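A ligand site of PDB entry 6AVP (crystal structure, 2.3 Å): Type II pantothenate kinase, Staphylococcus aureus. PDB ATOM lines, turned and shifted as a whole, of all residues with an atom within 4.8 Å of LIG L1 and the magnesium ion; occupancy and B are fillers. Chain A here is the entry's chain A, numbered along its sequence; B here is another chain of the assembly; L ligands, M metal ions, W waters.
Merely in contact with the magnesium ion: Asp 6 (3.9 Å) and Lys 13 (3.96 Å).
Water W6 lies within hydrogen-bond range of the side-chain amide nitrogen of Asn 96 and the side-chain carboxylate of Glu 70. Water W1 lies within hydrogen-bond range of OD2 of Asp 6 and NZ of Lys 13. Water W4 bridges OD1 of Asn 96 (2.8 Å) and O4 of LG2 L2 (3.1 Å). Water W2 lies within hydrogen-bond range of the side-chain carboxylate of Asp 6 (2.7 Å) and the side-chain carboxylate of Glu 70 (3.3 Å). Water W5 lies within hydrogen-bond range of the side-chain hydroxyl of Thr 206 of chain B (2.5 Å), the side-chain hydroxyl of Tyr 240 of chain B (2.7 Å) and the backbone carbonyl oxygen of Gly 116 (3.0 Å).
The magnesium ion is bound by O2 of LG2 L2 (1.9 Å), water W2 (2.0 Å), water W1 (2.0 Å), O2 of LIG L1 (2.2 Å), water W4 (2.2 Å) and water W6 (2.4 Å).
The backbone NH (N) of Thr 99 is in hydrogen-bond range of an oxygen (O1) of LIG L1 (3.5 Å). A nitrogen (N2) of LIG L1 sits at hydrogen-bond distance from the backbone carbonyl oxygen (O) of Thr 172 of chain B (2.8 Å). N of Gly 100 is in hydrogen-bond range of O1 of LIG L1 (3.0 Å). O1 of LG2 L2 sits at hydrogen-bond distance from N of Gly 9 (2.9 Å). The side-chain hydroxyl (OG1) of Thr 172 of chain B sits at hydrogen-bond distance from an oxygen (O8) of LIG L1. A nitrogen (N1) of LIG L1 sits at hydrogen-bond distance from the backbone carbonyl oxygen (O) of Ala 173 of chain B (3.3 Å). The side-chain hydroxyl of Thr 99 is in hydrogen-bond range of an oxygen (O1) of LG2 L2, at 2.6 Å. An oxygen (O8) of LIG L1 is in hydrogen-bond range of the backbone NH of Thr 172 of chain B (3.0 Å). An oxygen (O7) of LIG L1 sits at hydrogen-bond distance from the guanidinium group (NH2) of Arg 113, at 2.8 Å. N of Thr 99 lies within hydrogen-bond range of O6 of LG2 L2 (3.1 Å). O5 of LG2 L2 is in salt-bridge range of NZ of Lys 13.
The backbone carbonyl oxygen (O) of Asp 6 sits at hydrogen-bond distance from the backbone NH (N) of Lys 13 (2.9 Å). N of Asn 96 lies within hydrogen-bond range of O of Ser 102 (2.9 Å). OH of Tyr 160 of chain B lies within hydrogen-bond range of OE2 of Glu 70, at 2.6 Å. O of Leu 171 of chain B is in hydrogen-bond range of N of Val 156 of chain B (3.0 Å). The backbone carbonyl oxygen (O) of Glu 202 of chain B is in hydrogen-bond range of the side-chain hydroxyl (OG1) of Thr 206 of chain B (2.7 Å). The side-chain hydroxyl (OG1) of Thr 172 of chain B is in hydrogen-bond range of the side-chain carboxylate (OE2) of Glu 202 of chain B. The backbone carbonyl oxygen of Thr 101 lies within hydrogen-bond range of the backbone NH of Ile 117, at 3.0 Å. The guanidinium group of Arg 113 lies within hydrogen-bond range of the side-chain hydroxyl of Ser 102 (2.7 Å).
OE1 of Glu 70 lies close to O4 of LIG L1 (3.3 Å). An oxygen (O6) of LIG L1 lies close to the backbone carbonyl oxygen (O) of Thr 101, at 3.3 Å. O7 of LIG L1 sits close to O of Gly 116, 3.4 Å away. Gly 9 touches LIG L1 (N to O3, 3.6 Å). Phe 71 touches LIG L1. Gly 98 touches LIG L1 (C to O1, 3.98 Å). Ser 102 touches LIG L1 (CB to O6, 3.6 Å). Ile 117 touches LIG L1. Val 156 of chain B touches LIG L1 (CG2 to C4, 3.8 Å). Ile 159 of chain B touches LIG L1. Leu 171 of chain B touches LIG L1 (CA to O8, 3.7 Å). Glu 202 of chain B touches LIG L1 (CD to C14, 3.7 Å). Tyr 240 of chain B touches LIG L1 (CZ to C12, 3.3 Å). Hydrophobic or aromatic side chains that line LIG L1: Phe 71, Val 156 of chain B, Ile 159 of chain B, Leu 171 of chain B and Tyr 240 of chain B. Of the 27 residues printed, 18 come within 4 Å of LIG L1. The nearest printed residue that does not touch LIG L1 is Ile 167 of chain B (4.01 Å).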
ATOM      1  N   ASP A   6     -27.987  25.975  11.396  1.00  0.00           N
ATOM      2  CA  ASP A   6     -27.345  24.771  10.863  1.00  0.00           C
ATOM      3  C   ASP A   6     -26.181  24.470  11.802  1.00  0.00           C
ATOM      4  O   ASP A   6     -25.164  25.162  11.769  1.00  0.00           O
ATOM      5  CB  ASP A   6     -26.861  25.032   9.439  1.00  0.00           C
ATOM      6  CG  ASP A   6     -26.121  23.844   8.816  1.00  0.00           C
ATOM      7  OD1 ASP A   6     -25.704  22.909   9.533  1.00  0.00           O
ATOM      8  OD2 ASP A   6     -25.934  23.841   7.581  1.00  0.00           O
ATOM      9  N   GLY A   8     -23.390  22.337  12.500  1.00  0.00           N
ATOM     10  CA  GLY A   8     -22.537  21.373  11.827  1.00  0.00           C
ATOM     11  C   GLY A   8     -21.486  20.771  12.728  1.00  0.00           C
ATOM     12  O   GLY A   8     -21.501  20.945  13.956  1.00  0.00           O
ATOM     13  N   GLY A   9     -20.587  20.036  12.081  1.00  0.00           N
ATOM     14  CA  GLY A   9     -19.523  19.316  12.755  1.00  0.00           C
ATOM     15  C   GLY A   9     -18.486  20.217  13.375  1.00  0.00           C
ATOM     16  O   GLY A   9     -17.912  19.870  14.402  1.00  0.00           O
ATOM     17  N   LYS A  13     -24.043  27.822  12.327  1.00  0.00           N
ATOM     18  CA  LYS A  13     -24.434  28.998  11.543  1.00  0.00           C
ATOM     19  C   LYS A  13     -25.823  29.405  11.931  1.00  0.00           C
ATOM     20  O   LYS A  13     -26.733  28.606  11.921  1.00  0.00           O
ATOM     21  CB  LYS A  13     -24.413  28.752  10.043  1.00  0.00           C
ATOM     22  CG  LYS A  13     -23.042  28.471   9.472  1.00  0.00           C
ATOM     23  CD  LYS A  13     -22.945  27.011   9.066  1.00  0.00           C
ATOM     24  CE  LYS A  13     -21.812  26.304   9.737  1.00  0.00           C
ATOM     25  NZ  LYS A  13     -21.958  24.821   9.662  1.00  0.00           N
ATOM     26  N   GLU A  70     -30.451  18.301   6.666  1.00  0.00           N
ATOM     27  CA  GLU A  70     -29.536  19.346   6.146  1.00  0.00           C
ATOM     28  C   GLU A  70     -29.353  19.384   4.621  1.00  0.00           C
ATOM     29  O   GLU A  70     -28.988  20.445   4.080  1.00  0.00           O
ATOM     30  CB  GLU A  70     -28.150  19.251   6.819  1.00  0.00           C
ATOM     31  CG  GLU A  70     -27.349  17.975   6.572  1.00  0.00           C
ATOM     32  CD  GLU A  70     -25.890  18.085   7.008  1.00  0.00           C
ATOM     33  OE1 GLU A  70     -25.064  18.529   6.190  1.00  0.00           O
ATOM     34  OE2 GLU A  70     -25.555  17.719   8.159  1.00  0.00           O
ATOM     35  N   PHE A  71     -29.577  18.262   3.960  1.00  0.00           N
ATOM     36  CA  PHE A  71     -29.512  18.200   2.494  1.00  0.00           C
ATOM     37  C   PHE A  71     -30.667  18.987   1.881  1.00  0.00           C
ATOM     38  O   PHE A  71     -30.468  19.797   0.972  1.00  0.00           O
ATOM     39  CB  PHE A  71     -29.563  16.750   1.988  1.00  0.00           C
ATOM     40  CG  PHE A  71     -28.476  15.866   2.538  1.00  0.00           C
ATOM     41  CD1 PHE A  71     -27.191  16.347   2.785  1.00  0.00           C
ATOM     42  CD2 PHE A  71     -28.722  14.519   2.771  1.00  0.00           C
ATOM     43  CE1 PHE A  71     -26.189  15.515   3.272  1.00  0.00           C
ATOM     44  CE2 PHE A  71     -27.734  13.678   3.260  1.00  0.00           C
ATOM     45  CZ  PHE A  71     -26.456  14.180   3.511  1.00  0.00           C
ATOM     46  N   ASN A  96     -21.317  20.771  -1.205  1.00  0.00           N
ATOM     47  CA  ASN A  96     -21.202  21.369   0.134  1.00  0.00           C
ATOM     48  C   ASN A  96     -19.884  20.927   0.796  1.00  0.00           C
ATOM     49  O   ASN A  96     -19.749  19.780   1.266  1.00  0.00           O
ATOM     50  CB  ASN A  96     -22.380  20.888   0.949  1.00  0.00           C
ATOM     51  CG  ASN A  96     -22.605  21.691   2.189  1.00  0.00           C
ATOM     52  OD1 ASN A  96     -21.690  22.319   2.720  1.00  0.00           O
ATOM     53  ND2 ASN A  96     -23.829  21.704   2.644  1.00  0.00           N
ATOM     54  N   GLY A  98     -17.856  21.128   3.652  1.00  0.00           N
ATOM     55  CA  GLY A  98     -17.869  21.456   5.089  1.00  0.00           C
ATOM     56  C   GLY A  98     -16.773  20.715   5.814  1.00  0.00           C
ATOM     57  O   GLY A  98     -15.700  20.494   5.243  1.00  0.00           O
ATOM     58  N   THR A  99     -17.013  20.338   7.068  1.00  0.00           N
ATOM     59  CA  THR A  99     -16.092  19.450   7.762  1.00  0.00           C
ATOM     60  C   THR A  99     -15.795  18.242   6.861  1.00  0.00           C
ATOM     61  O   THR A  99     -14.653  17.810   6.780  1.00  0.00           O
ATOM     62  CB  THR A  99     -16.678  18.946   9.091  1.00  0.00           C
ATOM     63  OG1 THR A  99     -17.103  20.059   9.883  1.00  0.00           O
ATOM     64  CG2 THR A  99     -15.653  18.147   9.861  1.00  0.00           C
ATOM     65  N   GLY A 100     -16.861  17.698   6.261  1.00  0.00           N
ATOM     66  CA  GLY A 100     -16.806  16.701   5.200  1.00  0.00           C
ATOM     67  C   GLY A 100     -17.484  17.252   3.944  1.00  0.00           C
ATOM     68  O   GLY A 100     -17.895  18.386   3.916  1.00  0.00           O
ATOM     69  N   THR A 101     -17.614  16.445   2.896  1.00  0.00           N
ATOM     70  CA  THR A 101     -18.135  16.924   1.604  1.00  0.00           C
ATOM     71  C   THR A 101     -19.281  16.051   1.071  1.00  0.00           C
ATOM     72  O   THR A 101     -19.178  14.825   0.986  1.00  0.00           O
ATOM     73  CB  THR A 101     -17.007  17.044   0.582  1.00  0.00           C
ATOM     74  OG1 THR A 101     -16.058  17.980   1.066  1.00  0.00           O
ATOM     75  CG2 THR A 101     -17.502  17.550  -0.770  1.00  0.00           C
ATOM     76  N   SER A 102     -20.363  16.715   0.707  1.00  0.00           N
ATOM     77  CA  SER A 102     -21.588  16.105   0.215  1.00  0.00           C
ATOM     78  C   SER A 102     -21.917  16.682  -1.164  1.00  0.00           C
ATOM     79  O   SER A 102     -21.935  17.915  -1.332  1.00  0.00           O
ATOM     80  CB  SER A 102     -22.717  16.430   1.203  1.00  0.00           C
ATOM     81  OG  SER A 102     -23.799  15.556   1.005  1.00  0.00           O
ATOM     82  N   ARG A 113     -28.931  13.678  -3.349  1.00  0.00           N
ATOM     83  CA  ARG A 113     -27.543  13.422  -3.030  1.00  0.00           C
ATOM     84  C   ARG A 113     -27.015  12.407  -4.033  1.00  0.00           C
ATOM     85  O   ARG A 113     -27.617  11.358  -4.212  1.00  0.00           O
ATOM     86  CB  ARG A 113     -27.377  12.887  -1.616  1.00  0.00           C
ATOM     87  CG  ARG A 113     -25.924  12.830  -1.184  1.00  0.00           C
ATOM     88  CD  ARG A 113     -25.774  12.781   0.335  1.00  0.00           C
ATOM     89  NE  ARG A 113     -24.377  12.910   0.741  1.00  0.00           N
ATOM     90  CZ  ARG A 113     -23.495  11.911   0.846  1.00  0.00           C
ATOM     91  NH1 ARG A 113     -23.837  10.655   0.612  1.00  0.00           N
ATOM     92  NH2 ARG A 113     -22.257  12.162   1.234  1.00  0.00           N
ATOM     93  N   GLY A 116     -20.452  11.701  -2.054  1.00  0.00           N
ATOM     94  CA  GLY A 116     -19.727  12.515  -1.137  1.00  0.00           C
ATOM     95  C   GLY A 116     -18.415  11.872  -0.832  1.00  0.00           C
ATOM     96  O   GLY A 116     -18.198  10.691  -1.104  1.00  0.00           O
ATOM     97  N   ILE A 117     -17.550  12.680  -0.250  1.00  0.00           N
ATOM     98  CA  ILE A 117     -16.227  12.242   0.104  1.00  0.00           C
ATOM     99  C   ILE A 117     -15.795  12.921   1.391  1.00  0.00           C
ATOM    100  O   ILE A 117     -16.263  14.015   1.706  1.00  0.00           O
ATOM    101  CB  ILE A 117     -15.307  12.529  -1.086  1.00  0.00           C
ATOM    102  CG1 ILE A 117     -13.905  11.966  -0.868  1.00  0.00           C
ATOM    103  CG2 ILE A 117     -15.272  14.014  -1.397  1.00  0.00           C
ATOM    104  CD1 ILE A 117     -13.842  10.446  -0.883  1.00  0.00           C
ATOM    105  N   GLY A 118     -14.895  12.285   2.134  1.00  0.00           N
ATOM    106  CA  GLY A 118     -14.349  12.863   3.360  1.00  0.00           C
ATOM    107  C   GLY A 118     -13.201  13.869   3.221  1.00  0.00           C
ATOM    108  O   GLY A 118     -12.623  14.272   4.223  1.00  0.00           O
ATOM    109  N   VAL B 156     -19.581   9.762  10.381  1.00  0.00           N
ATOM    110  CA  VAL B 156     -20.858  10.471  10.252  1.00  0.00           C
ATOM    111  C   VAL B 156     -21.567  10.484  11.607  1.00  0.00           C
ATOM    112  O   VAL B 156     -22.126  11.497  12.009  1.00  0.00           O
ATOM    113  CB  VAL B 156     -21.720   9.847   9.134  1.00  0.00           C
ATOM    114  CG1 VAL B 156     -23.152  10.380   9.151  1.00  0.00           C
ATOM    115  CG2 VAL B 156     -21.079  10.097   7.780  1.00  0.00           C
ATOM    116  N   ILE B 159     -20.378  13.440  13.958  1.00  0.00           N
ATOM    117  CA  ILE B 159     -21.021  14.725  13.659  1.00  0.00           C
ATOM    118  C   ILE B 159     -22.470  14.704  14.150  1.00  0.00           C
ATOM    119  O   ILE B 159     -22.957  15.680  14.670  1.00  0.00           O
ATOM    120  CB  ILE B 159     -20.964  15.062  12.144  1.00  0.00           C
ATOM    121  CG1 ILE B 159     -19.536  15.455  11.759  1.00  0.00           C
ATOM    122  CG2 ILE B 159     -21.910  16.198  11.775  1.00  0.00           C
ATOM    123  CD1 ILE B 159     -19.305  15.612  10.274  1.00  0.00           C
ATOM    124  N   TYR B 160     -23.143  13.571  13.963  1.00  0.00           N
ATOM    125  CA  TYR B 160     -24.565  13.414  14.272  1.00  0.00           C
ATOM    126  C   TYR B 160     -24.797  12.742  15.616  1.00  0.00           C
ATOM    127  O   TYR B 160     -25.397  11.658  15.704  1.00  0.00           O
ATOM    128  CB  TYR B 160     -25.245  12.597  13.183  1.00  0.00           C
ATOM    129  CG  TYR B 160     -25.721  13.441  12.053  1.00  0.00           C
ATOM    130  CD1 TYR B 160     -24.862  13.771  11.017  1.00  0.00           C
ATOM    131  CD2 TYR B 160     -27.022  13.902  12.013  1.00  0.00           C
ATOM    132  CE1 TYR B 160     -25.296  14.550   9.974  1.00  0.00           C
ATOM    133  CE2 TYR B 160     -27.476  14.676  10.961  1.00  0.00           C
ATOM    134  CZ  TYR B 160     -26.595  15.003   9.955  1.00  0.00           C
ATOM    135  OH  TYR B 160     -27.020  15.770   8.912  1.00  0.00           O
ATOM    136  N   ILE B 167     -27.489   9.652   6.277  1.00  0.00           N
ATOM    137  CA  ILE B 167     -26.703   8.600   5.610  1.00  0.00           C
ATOM    138  C   ILE B 167     -26.089   7.713   6.716  1.00  0.00           C
ATOM    139  O   ILE B 167     -26.030   8.144   7.876  1.00  0.00           O
ATOM    140  CB  ILE B 167     -25.608   9.211   4.687  1.00  0.00           C
ATOM    141  CG1 ILE B 167     -24.707  10.199   5.455  1.00  0.00           C
ATOM    142  CG2 ILE B 167     -26.277   9.881   3.489  1.00  0.00           C
ATOM    143  CD1 ILE B 167     -23.472  10.649   4.710  1.00  0.00           C
ATOM    144  N   ASP B 170     -21.647   4.913  10.128  1.00  0.00           N
ATOM    145  CA  ASP B 170     -20.339   4.328  10.025  1.00  0.00           C
ATOM    146  C   ASP B 170     -19.485   4.888   8.873  1.00  0.00           C
ATOM    147  O   ASP B 170     -18.281   4.652   8.847  1.00  0.00           O
ATOM    148  CB  ASP B 170     -20.429   2.807   9.883  1.00  0.00           C
ATOM    149  CG  ASP B 170     -19.093   2.139  10.091  1.00  0.00           C
ATOM    150  OD1 ASP B 170     -18.579   2.153  11.238  1.00  0.00           O
ATOM    151  OD2 ASP B 170     -18.518   1.646   9.095  1.00  0.00           O
ATOM    152  N   LEU B 171     -20.103   5.599   7.916  1.00  0.00           N
ATOM    153  CA  LEU B 171     -19.314   6.215   6.843  1.00  0.00           C
ATOM    154  C   LEU B 171     -18.260   7.145   7.433  1.00  0.00           C
ATOM    155  O   LEU B 171     -18.451   7.697   8.518  1.00  0.00           O
ATOM    156  CB  LEU B 171     -20.203   7.007   5.880  1.00  0.00           C
ATOM    157  CG  LEU B 171     -21.082   6.233   4.902  1.00  0.00           C
ATOM    158  CD1 LEU B 171     -22.139   7.130   4.268  1.00  0.00           C
ATOM    159  CD2 LEU B 171     -20.233   5.594   3.818  1.00  0.00           C
ATOM    160  N   THR B 172     -17.117   7.240   6.743  1.00  0.00           N
ATOM    161  CA  THR B 172     -16.137   8.284   7.014  1.00  0.00           C
ATOM    162  C   THR B 172     -16.794   9.576   6.534  1.00  0.00           C
ATOM    163  O   THR B 172     -17.349   9.636   5.435  1.00  0.00           O
ATOM    164  CB  THR B 172     -14.790   8.064   6.262  1.00  0.00           C
ATOM    165  OG1 THR B 172     -14.213   6.795   6.606  1.00  0.00           O
ATOM    166  CG2 THR B 172     -13.784   9.134   6.606  1.00  0.00           C
ATOM    167  N   ALA B 173     -16.721  10.593   7.384  1.00  0.00           N
ATOM    168  CA  ALA B 173     -17.252  11.929   7.110  1.00  0.00           C
ATOM    169  C   ALA B 173     -16.156  12.875   6.690  1.00  0.00           C
ATOM    170  O   ALA B 173     -16.335  13.622   5.738  1.00  0.00           O
ATOM    171  CB  ALA B 173     -17.941  12.497   8.348  1.00  0.00           C
ATOM    172  N   GLU B 202     -10.411   5.397  -0.113  1.00  0.00           N
ATOM    173  CA  GLU B 202     -11.763   5.882  -0.144  1.00  0.00           C
ATOM    174  C   GLU B 202     -12.017   6.785  -1.348  1.00  0.00           C
ATOM    175  O   GLU B 202     -13.102   6.752  -1.915  1.00  0.00           O
ATOM    176  CB  GLU B 202     -12.098   6.616   1.156  1.00  0.00           C
ATOM    177  CG  GLU B 202     -12.257   5.678   2.344  1.00  0.00           C
ATOM    178  CD  GLU B 202     -12.544   6.393   3.680  1.00  0.00           C
ATOM    179  OE1 GLU B 202     -12.908   7.594   3.689  1.00  0.00           O
ATOM    180  OE2 GLU B 202     -12.396   5.744   4.735  1.00  0.00           O
ATOM    181  N   THR B 206     -14.666   5.847  -4.294  1.00  0.00           N
ATOM    182  CA  THR B 206     -15.738   6.775  -4.593  1.00  0.00           C
ATOM    183  C   THR B 206     -15.748   7.135  -6.084  1.00  0.00           C
ATOM    184  O   THR B 206     -16.802   7.115  -6.735  1.00  0.00           O
ATOM    185  CB  THR B 206     -15.617   8.041  -3.745  1.00  0.00           C
ATOM    186  OG1 THR B 206     -15.595   7.673  -2.363  1.00  0.00           O
ATOM    187  CG2 THR B 206     -16.785   8.946  -3.966  1.00  0.00           C
ATOM    188  N   TYR B 240     -15.767  -1.004   1.012  1.00  0.00           N
ATOM    189  CA  TYR B 240     -16.578   0.088   0.561  1.00  0.00           C
ATOM    190  C   TYR B 240     -17.138  -0.112  -0.844  1.00  0.00           C
ATOM    191  O   TYR B 240     -18.232   0.363  -1.109  1.00  0.00           O
ATOM    192  CB  TYR B 240     -15.824   1.423   0.679  1.00  0.00           C
ATOM    193  CG  TYR B 240     -16.740   2.612   0.491  1.00  0.00           C
ATOM    194  CD1 TYR B 240     -17.921   2.741   1.227  1.00  0.00           C
ATOM    195  CD2 TYR B 240     -16.441   3.604  -0.428  1.00  0.00           C
ATOM    196  CE1 TYR B 240     -18.772   3.804   1.041  1.00  0.00           C
ATOM    197  CE2 TYR B 240     -17.295   4.691  -0.620  1.00  0.00           C
ATOM    198  CZ  TYR B 240     -18.466   4.774   0.119  1.00  0.00           C
ATOM    199  OH  TYR B 240     -19.315   5.847  -0.031  1.00  0.00           O
HETATM  200  O1  LIG L   1     -19.755  18.252   6.742  1.00  0.00           O
HETATM  201  P1  LIG L   1     -21.030  18.702   7.440  1.00  0.00           P
HETATM  202  O2  LIG L   1     -21.789  19.830   6.887  1.00  0.00           O
HETATM  203  O3  LIG L   1     -21.158  18.479   8.892  1.00  0.00           O
HETATM  204  O4  LIG L   1     -22.047  17.522   6.918  1.00  0.00           O
HETATM  205  C1  LIG L   1     -21.931  16.166   7.424  1.00  0.00           C
HETATM  206  C2  LIG L   1     -21.879  15.098   6.287  1.00  0.00           C
HETATM  207  C3  LIG L   1     -23.222  15.112   5.521  1.00  0.00           C
HETATM  208  C4  LIG L   1     -21.634  13.736   6.952  1.00  0.00           C
HETATM  209  C5  LIG L   1     -20.725  15.443   5.315  1.00  0.00           C
HETATM  210  O5  LIG L   1     -19.546  15.660   6.058  1.00  0.00           O
HETATM  211  C6  LIG L   1     -20.482  14.326   4.284  1.00  0.00           C
HETATM  212  O6  LIG L   1     -21.316  14.038   3.424  1.00  0.00           O
HETATM  213  N1  LIG L   1     -19.343  13.659   4.503  1.00  0.00           N
HETATM  214  C7  LIG L   1     -18.850  12.576   3.657  1.00  0.00           C
HETATM  215  C8  LIG L   1     -19.592  11.291   3.934  1.00  0.00           C
HETATM  216  C9  LIG L   1     -19.332  10.376   2.733  1.00  0.00           C
HETATM  217  O7  LIG L   1     -20.036  10.487   1.733  1.00  0.00           O
HETATM  218  N2  LIG L   1     -18.294   9.519   2.827  1.00  0.00           N
HETATM  219  C10 LIG L   1     -18.077   8.565   1.764  1.00  0.00           C
HETATM  220  C11 LIG L   1     -16.618   8.266   1.633  1.00  0.00           C
HETATM  221  C12 LIG L   1     -16.426   6.757   1.860  1.00  0.00           C
HETATM  222  C13 LIG L   1     -16.475   6.502   3.345  1.00  0.00           C
HETATM  223  C14 LIG L   1     -16.043   5.073   3.588  1.00  0.00           C
HETATM  224  O8  LIG L   1     -16.347   4.850   5.015  1.00  0.00           O
HETATM  225  C15 LIG L   1     -15.775   3.661   5.568  1.00  0.00           C
HETATM  226  P1  LG2 L   2     -19.998  22.129   9.160  1.00  0.00           P
HETATM  227  O1  LG2 L   2     -19.609  20.687   9.394  1.00  0.00           O
HETATM  228  O2  LG2 L   2     -21.383  22.310   8.579  1.00  0.00           O
HETATM  229  O3  LG2 L   2     -19.721  23.011  10.342  1.00  0.00           O
HETATM  230  P2  LG2 L   2     -18.777  24.145   7.520  1.00  0.00           P
HETATM  231  O4  LG2 L   2     -19.052  24.313   6.040  1.00  0.00           O
HETATM  232  O5  LG2 L   2     -19.464  25.058   8.476  1.00  0.00           O
HETATM  233  O6  LG2 L   2     -18.972  22.608   7.987  1.00  0.00           O
HETATM  234  O7  LG2 L   2     -17.212  24.476   7.659  1.00  0.00           O
HETATM  235  C1  LG2 L   2     -16.213  23.719   8.308  1.00  0.00           C
HETATM  236  C2  LG2 L   2     -14.857  24.139   7.768  1.00  0.00           C
HETATM  237  O8  LG2 L   2     -14.724  25.530   7.481  1.00  0.00           O
HETATM  238  C3  LG2 L   2     -13.740  23.824   8.740  1.00  0.00           C
HETATM  239  O9  LG2 L   2     -13.477  22.416   8.724  1.00  0.00           O
HETATM  240  C4  LG2 L   2     -12.616  24.712   8.227  1.00  0.00           C
HETATM  241  O10 LG2 L   2     -11.892  24.125   7.131  1.00  0.00           O
HETATM  242  C5  LG2 L   2     -13.358  25.946   7.698  1.00  0.00           C
HETATM  243  N1  LG2 L   2     -13.403  27.131   8.603  1.00  0.00           N
HETATM  244  C6  LG2 L   2     -13.760  28.355   8.178  1.00  0.00           C
HETATM  245  N2  LG2 L   2     -13.749  29.243   9.191  1.00  0.00           N
HETATM  246  C7  LG2 L   2     -13.418  28.582  10.303  1.00  0.00           C
HETATM  247  C8  LG2 L   2     -13.240  28.931  11.732  1.00  0.00           C
HETATM  248  N3  LG2 L   2     -13.427  30.201  12.173  1.00  0.00           N
HETATM  249  N4  LG2 L   2     -12.879  27.940  12.577  1.00  0.00           N
HETATM  250  C9  LG2 L   2     -12.698  26.675  12.158  1.00  0.00           C
HETATM  251  N5  LG2 L   2     -12.852  26.317  10.880  1.00  0.00           N
HETATM  252  C10 LG2 L   2     -13.193  27.193   9.922  1.00  0.00           C
HETATM  253 MG    MG M   1     -22.622  21.822   7.162  1.00  0.00          MG
HETATM  254  O   HOH W   1     -23.293  23.712   7.261  1.00  0.00           O
HETATM  255  O   HOH W   2     -24.238  21.100   8.082  1.00  0.00           O
HETATM  256  O   HOH W   3     -20.857  19.435   4.174  1.00  0.00           O
HETATM  257  O   HOH W   4     -21.268  22.264   5.485  1.00  0.00           O
HETATM  258  O   HOH W   5     -17.944   7.750  -1.389  1.00  0.00           O
HETATM  259  O   HOH W   6     -23.685  21.046   5.192  1.00  0.00           O
